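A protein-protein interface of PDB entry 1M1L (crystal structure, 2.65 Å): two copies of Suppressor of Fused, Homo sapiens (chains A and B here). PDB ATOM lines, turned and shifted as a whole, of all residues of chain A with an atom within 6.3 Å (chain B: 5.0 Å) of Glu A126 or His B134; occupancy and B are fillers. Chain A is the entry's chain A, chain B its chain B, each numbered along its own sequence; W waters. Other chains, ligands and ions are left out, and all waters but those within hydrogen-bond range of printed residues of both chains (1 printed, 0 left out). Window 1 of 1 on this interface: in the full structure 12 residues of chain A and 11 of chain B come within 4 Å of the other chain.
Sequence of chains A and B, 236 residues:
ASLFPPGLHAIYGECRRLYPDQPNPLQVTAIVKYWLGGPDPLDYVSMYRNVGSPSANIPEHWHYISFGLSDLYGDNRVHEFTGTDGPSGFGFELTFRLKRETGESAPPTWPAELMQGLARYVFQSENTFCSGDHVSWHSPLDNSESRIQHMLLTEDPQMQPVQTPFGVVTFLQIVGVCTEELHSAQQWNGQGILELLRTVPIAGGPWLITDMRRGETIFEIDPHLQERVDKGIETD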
ATOM      1  N   PHE A  90      -3.580  -1.902 -22.297  1.00  0.00           N
ATOM      2  CA  PHE A  90      -3.031  -1.660 -23.618  1.00  0.00           C
ATOM      3  C   PHE A  90      -2.129  -0.430 -23.677  1.00  0.00           C
ATOM      4  O   PHE A  90      -1.542  -0.125 -24.721  1.00  0.00           O
ATOM      5  CB  PHE A  90      -4.155  -1.539 -24.630  1.00  0.00           C
ATOM      6  CG  PHE A  90      -4.768  -2.857 -24.985  1.00  0.00           C
ATOM      7  CD1 PHE A  90      -6.043  -3.191 -24.535  1.00  0.00           C
ATOM      8  CD2 PHE A  90      -4.051  -3.786 -25.748  1.00  0.00           C
ATOM      9  CE1 PHE A  90      -6.601  -4.438 -24.839  1.00  0.00           C
ATOM     10  CE2 PHE A  90      -4.594  -5.028 -26.054  1.00  0.00           C
ATOM     11  CZ  PHE A  90      -5.874  -5.357 -25.600  1.00  0.00           C
ATOM     12  N   TYR A 121     -11.732  -3.678 -31.578  1.00  0.00           N
ATOM     13  CA  TYR A 121     -10.637  -4.133 -32.431  1.00  0.00           C
ATOM     14  C   TYR A 121      -9.366  -4.409 -31.619  1.00  0.00           C
ATOM     15  O   TYR A 121      -8.664  -5.385 -31.865  1.00  0.00           O
ATOM     16  CB  TYR A 121     -10.320  -3.080 -33.508  1.00  0.00           C
ATOM     17  CG  TYR A 121     -11.397  -2.921 -34.561  1.00  0.00           C
ATOM     18  CD1 TYR A 121     -11.337  -1.905 -35.501  1.00  0.00           C
ATOM     19  CD2 TYR A 121     -12.472  -3.799 -34.638  1.00  0.00           C
ATOM     20  CE1 TYR A 121     -12.336  -1.774 -36.506  1.00  0.00           C
ATOM     21  CE2 TYR A 121     -13.461  -3.664 -35.633  1.00  0.00           C
ATOM     22  CZ  TYR A 121     -13.388  -2.660 -36.561  1.00  0.00           C
ATOM     23  OH  TYR A 121     -14.362  -2.570 -37.548  1.00  0.00           O
ATOM     24  N   VAL A 122      -9.072  -3.538 -30.656  1.00  0.00           N
ATOM     25  CA  VAL A 122      -7.876  -3.683 -29.834  1.00  0.00           C
ATOM     26  C   VAL A 122      -7.966  -4.910 -28.926  1.00  0.00           C
ATOM     27  O   VAL A 122      -7.040  -5.725 -28.883  1.00  0.00           O
ATOM     28  CB  VAL A 122      -7.600  -2.369 -29.015  1.00  0.00           C
ATOM     29  CG1 VAL A 122      -6.409  -2.533 -28.085  1.00  0.00           C
ATOM     30  CG2 VAL A 122      -7.310  -1.230 -29.978  1.00  0.00           C
ATOM     31  N   PHE A 123      -9.079  -5.062 -28.222  1.00  0.00           N
ATOM     32  CA  PHE A 123      -9.252  -6.209 -27.343  1.00  0.00           C
ATOM     33  C   PHE A 123      -9.216  -7.551 -28.088  1.00  0.00           C
ATOM     34  O   PHE A 123      -8.542  -8.487 -27.657  1.00  0.00           O
ATOM     35  CB  PHE A 123     -10.583  -6.122 -26.585  1.00  0.00           C
ATOM     36  CG  PHE A 123     -10.543  -5.274 -25.344  1.00  0.00           C
ATOM     37  CD1 PHE A 123     -10.459  -3.884 -25.422  1.00  0.00           C
ATOM     38  CD2 PHE A 123     -10.628  -5.866 -24.088  1.00  0.00           C
ATOM     39  CE1 PHE A 123     -10.466  -3.097 -24.255  1.00  0.00           C
ATOM     40  CE2 PHE A 123     -10.635  -5.091 -22.917  1.00  0.00           C
ATOM     41  CZ  PHE A 123     -10.555  -3.708 -23.002  1.00  0.00           C
ATOM     42  N   GLN A 124      -9.953  -7.646 -29.194  1.00  0.00           N
ATOM     43  CA  GLN A 124     -10.036  -8.886 -29.964  1.00  0.00           C
ATOM     44  C   GLN A 124      -8.703  -9.317 -30.529  1.00  0.00           C
ATOM     45  O   GLN A 124      -8.227 -10.410 -30.243  1.00  0.00           O
ATOM     46  CB  GLN A 124     -10.991  -8.751 -31.152  1.00  0.00           C
ATOM     47  CG  GLN A 124     -12.237  -7.918 -30.940  1.00  0.00           C
ATOM     48  CD  GLN A 124     -13.342  -8.652 -30.256  1.00  0.00           C
ATOM     49  OE1 GLN A 124     -13.849  -9.627 -30.786  1.00  0.00           O
ATOM     50  NE2 GLN A 124     -13.733  -8.189 -29.071  1.00  0.00           N
ATOM     51  N   SER A 125      -8.118  -8.450 -31.344  1.00  0.00           N
ATOM     52  CA  SER A 125      -6.854  -8.729 -32.017  1.00  0.00           C
ATOM     53  C   SER A 125      -5.615  -8.601 -31.147  1.00  0.00           C
ATOM     54  O   SER A 125      -4.570  -9.176 -31.462  1.00  0.00           O
ATOM     55  CB  SER A 125      -6.689  -7.794 -33.217  1.00  0.00           C
ATOM     56  OG  SER A 125      -6.392  -6.475 -32.782  1.00  0.00           O
ATOM     57  N   GLU A 126      -5.743  -7.846 -30.061  1.00  0.00           N
ATOM     58  CA  GLU A 126      -4.642  -7.573 -29.152  1.00  0.00           C
ATOM     59  C   GLU A 126      -3.523  -6.745 -29.795  1.00  0.00           C
ATOM     60  O   GLU A 126      -2.392  -6.734 -29.316  1.00  0.00           O
ATOM     61  CB  GLU A 126      -4.089  -8.862 -28.549  1.00  0.00           C
ATOM     62  CG  GLU A 126      -4.970  -9.398 -27.434  1.00  0.00           C
ATOM     63  CD  GLU A 126      -4.572 -10.785 -26.970  1.00  0.00           C
ATOM     64  OE1 GLU A 126      -3.358 -11.032 -26.801  1.00  0.00           O
ATOM     65  OE2 GLU A 126      -5.476 -11.627 -26.763  1.00  0.00           O
ATOM     66  N   ASN A 127      -3.842  -6.056 -30.884  1.00  0.00           N
ATOM     67  CA  ASN A 127      -2.884  -5.166 -31.521  1.00  0.00           C
ATOM     68  C   ASN A 127      -3.229  -3.754 -31.073  1.00  0.00           C
ATOM     69  O   ASN A 127      -4.366  -3.326 -31.223  1.00  0.00           O
ATOM     70  CB  ASN A 127      -2.985  -5.241 -33.038  1.00  0.00           C
ATOM     71  CG  ASN A 127      -2.413  -6.503 -33.572  1.00  0.00           C
ATOM     72  OD1 ASN A 127      -1.375  -6.967 -33.088  1.00  0.00           O
ATOM     73  ND2 ASN A 127      -3.066  -7.079 -34.577  1.00  0.00           N
ATOM     74  N   THR A 128      -2.271  -3.020 -30.530  1.00  0.00           N
ATOM     75  CA  THR A 128      -2.575  -1.672 -30.082  1.00  0.00           C
ATOM     76  C   THR A 128      -2.465  -0.651 -31.221  1.00  0.00           C
ATOM     77  O   THR A 128      -2.174  -0.999 -32.357  1.00  0.00           O
ATOM     78  CB  THR A 128      -1.638  -1.260 -28.925  1.00  0.00           C
ATOM     79  OG1 THR A 128      -0.299  -1.173 -29.415  1.00  0.00           O
ATOM     80  CG2 THR A 128      -1.669  -2.290 -27.807  1.00  0.00           C
ATOM     81  N   GLY B 132      -1.447 -19.635 -36.380  1.00  0.00           N
ATOM     82  CA  GLY B 132      -1.011 -19.524 -35.002  1.00  0.00           C
ATOM     83  C   GLY B 132      -1.581 -18.339 -34.225  1.00  0.00           C
ATOM     84  O   GLY B 132      -1.539 -18.315 -32.991  1.00  0.00           O
ATOM     85  N   ASP B 133      -2.103 -17.344 -34.932  1.00  0.00           N
ATOM     86  CA  ASP B 133      -2.680 -16.192 -34.252  1.00  0.00           C
ATOM     87  C   ASP B 133      -3.960 -16.589 -33.534  1.00  0.00           C
ATOM     88  O   ASP B 133      -4.582 -17.610 -33.862  1.00  0.00           O
ATOM     89  CB  ASP B 133      -3.018 -15.077 -35.250  1.00  0.00           C
ATOM     90  CG  ASP B 133      -1.804 -14.317 -35.697  1.00  0.00           C
ATOM     91  OD1 ASP B 133      -0.699 -14.612 -35.196  1.00  0.00           O
ATOM     92  OD2 ASP B 133      -1.959 -13.418 -36.549  1.00  0.00           O
ATOM     93  N   HIS B 134      -4.345 -15.790 -32.545  1.00  0.00           N
ATOM     94  CA  HIS B 134      -5.587 -16.040 -31.830  1.00  0.00           C
ATOM     95  C   HIS B 134      -6.401 -14.755 -31.879  1.00  0.00           C
ATOM     96  O   HIS B 134      -5.851 -13.666 -32.009  1.00  0.00           O
ATOM     97  CB  HIS B 134      -5.326 -16.430 -30.377  1.00  0.00           C
ATOM     98  CG  HIS B 134      -4.536 -15.419 -29.605  1.00  0.00           C
ATOM     99  ND1 HIS B 134      -3.156 -15.406 -29.590  1.00  0.00           N
ATOM    100  CD2 HIS B 134      -4.933 -14.387 -28.823  1.00  0.00           C
ATOM    101  CE1 HIS B 134      -2.738 -14.413 -28.829  1.00  0.00           C
ATOM    102  NE2 HIS B 134      -3.795 -13.778 -28.353  1.00  0.00           N
ATOM    103  N   VAL B 135      -7.716 -14.877 -31.828  1.00  0.00           N
ATOM    104  CA  VAL B 135      -8.554 -13.693 -31.830  1.00  0.00           C
ATOM    105  C   VAL B 135      -9.513 -13.834 -30.658  1.00  0.00           C
ATOM    106  O   VAL B 135     -10.294 -14.779 -30.599  1.00  0.00           O
ATOM    107  CB  VAL B 135      -9.364 -13.536 -33.147  1.00  0.00           C
ATOM    108  CG1 VAL B 135     -10.328 -12.357 -33.016  1.00  0.00           C
ATOM    109  CG2 VAL B 135      -8.428 -13.289 -34.324  1.00  0.00           C
ATOM    110  N   SER B 136      -9.458 -12.899 -29.720  1.00  0.00           N
ATOM    111  CA  SER B 136     -10.332 -12.963 -28.551  1.00  0.00           C
ATOM    112  C   SER B 136     -11.722 -12.438 -28.886  1.00  0.00           C
ATOM    113  O   SER B 136     -12.151 -11.414 -28.355  1.00  0.00           O
ATOM    114  CB  SER B 136      -9.733 -12.148 -27.407  1.00  0.00           C
ATOM    115  OG  SER B 136      -8.406 -12.580 -27.134  1.00  0.00           O
ATOM    116  N   MET B 151     -11.258 -17.584 -31.351  1.00  0.00           N
ATOM    117  CA  MET B 151     -10.708 -18.200 -32.536  1.00  0.00           C
ATOM    118  C   MET B 151      -9.190 -18.300 -32.584  1.00  0.00           C
ATOM    119  O   MET B 151      -8.461 -17.464 -32.031  1.00  0.00           O
ATOM    120  CB  MET B 151     -11.189 -17.436 -33.782  1.00  0.00           C
ATOM    121  CG  MET B 151     -12.686 -17.454 -34.024  1.00  0.00           C
ATOM    122  SD  MET B 151     -13.149 -16.376 -35.418  1.00  0.00           S
ATOM    123  CE  MET B 151     -13.354 -14.793 -34.584  1.00  0.00           C
ATOM    124  N   LEU B 152      -8.734 -19.358 -33.246  1.00  0.00           N
ATOM    125  CA  LEU B 152      -7.317 -19.581 -33.487  1.00  0.00           C
ATOM    126  C   LEU B 152      -7.305 -19.712 -35.002  1.00  0.00           C
ATOM    127  O   LEU B 152      -8.305 -20.120 -35.600  1.00  0.00           O
ATOM    128  CB  LEU B 152      -6.829 -20.879 -32.850  1.00  0.00           C
ATOM    129  CG  LEU B 152      -6.704 -20.909 -31.332  1.00  0.00           C
ATOM    130  CD1 LEU B 152      -6.028 -22.199 -30.894  1.00  0.00           C
ATOM    131  CD2 LEU B 152      -5.888 -19.734 -30.873  1.00  0.00           C
ATOM    132  N   LEU B 182      -8.177 -20.506 -25.310  1.00  0.00           N
ATOM    133  CA  LEU B 182      -7.571 -19.267 -25.776  1.00  0.00           C
ATOM    134  C   LEU B 182      -6.468 -18.846 -24.808  1.00  0.00           C
ATOM    135  O   LEU B 182      -5.361 -18.508 -25.225  1.00  0.00           O
ATOM    136  CB  LEU B 182      -8.599 -18.139 -25.854  1.00  0.00           C
ATOM    137  CG  LEU B 182      -7.954 -16.760 -26.069  1.00  0.00           C
ATOM    138  CD1 LEU B 182      -7.589 -16.596 -27.524  1.00  0.00           C
ATOM    139  CD2 LEU B 182      -8.913 -15.655 -25.645  1.00  0.00           C
ATOM    140  N   ALA B 185      -3.448 -20.741 -25.193  1.00  0.00           N
ATOM    141  CA  ALA B 185      -2.683 -20.311 -26.362  1.00  0.00           C
ATOM    142  C   ALA B 185      -1.851 -19.076 -26.039  1.00  0.00           C
ATOM    143  O   ALA B 185      -0.767 -18.892 -26.584  1.00  0.00           O
ATOM    144  CB  ALA B 185      -3.627 -20.003 -27.528  1.00  0.00           C
ATOM    145  N   GLN B 186      -2.382 -18.229 -25.164  1.00  0.00           N
ATOM    146  CA  GLN B 186      -1.698 -17.010 -24.765  1.00  0.00           C
ATOM    147  C   GLN B 186      -0.521 -17.319 -23.855  1.00  0.00           C
ATOM    148  O   GLN B 186       0.531 -16.707 -23.970  1.00  0.00           O
ATOM    149  CB  GLN B 186      -2.676 -16.066 -24.069  1.00  0.00           C
ATOM    150  CG  GLN B 186      -3.761 -15.578 -24.993  1.00  0.00           C
ATOM    151  CD  GLN B 186      -4.840 -14.795 -24.277  1.00  0.00           C
ATOM    152  OE1 GLN B 186      -5.407 -15.276 -23.292  1.00  0.00           O
ATOM    153  NE2 GLN B 186      -5.145 -13.590 -24.776  1.00  0.00           N
HETATM  154  O   HOH W   1      -4.587 -11.355 -33.443  1.00  0.00           O
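O of Gln A124 sits at hydrogen-bond distance from N of Ser B136, 2.8 Å away. The side-chain carboxylate of Glu A126 is in hydrogen-bond range of a ring nitrogen (NE2) of His B134. OE2 of Glu A126 lies within hydrogen-bond range of OG of Ser B136 (3.1 Å). OE2 of Glu A126 sits at hydrogen-bond distance from NE2 of Gln B186 (2.8 Å).
N of Val B135 lies within hydrogen-bond range of O of Met B151, 2.7 Å away.
Phe A123 touches Ser B136 (O to CB, 3.9 Å). Val B135 touches Gln A124 (CA to O, 3.7 Å).
Printed residues of chain B within 4 Å of Gln A124: Val B135 and Ser B136. Printed residues of chain B within 4 Å of Glu A126: His B134 (3.2 Å), Ser B136 (3.1 Å) and Gln B186 (2.8 Å). His B134 touches just one residue of chain A: Glu A126 (3.2 Å). Printed residues of chain A within 4 Å of Val B135: Gln A124 (3.7 Å). Of the printed residues of chain A, Ser B136 touches Phe A123, Gln A124 and Glu A126. The nearest printed residue of chain B that does not touch Glu A126 is Leu B182 (5.4 Å). The nearest residue of chain A that does not touch His B134 is Gln A124 (4.4 Å).
Printed residues of chain B that touch a printed residue of chain A: His B134, Val B135, Ser B136 and Gln B186. Hydrophobic or aromatic side chains of chain B that line the printed part of chain A: His B134 and Val B135. Among the printed residues, 6 pairs touch across the chains. Among the printed residues, no Asp or Glu carboxylate lies within 4 Å of a Lys or Arg side-chain nitrogen of the other chain.
No position is printed for both chains.
Water W1 bridges O of Ser A125 (2.9 Å) and O of His B134 (3.0 Å).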
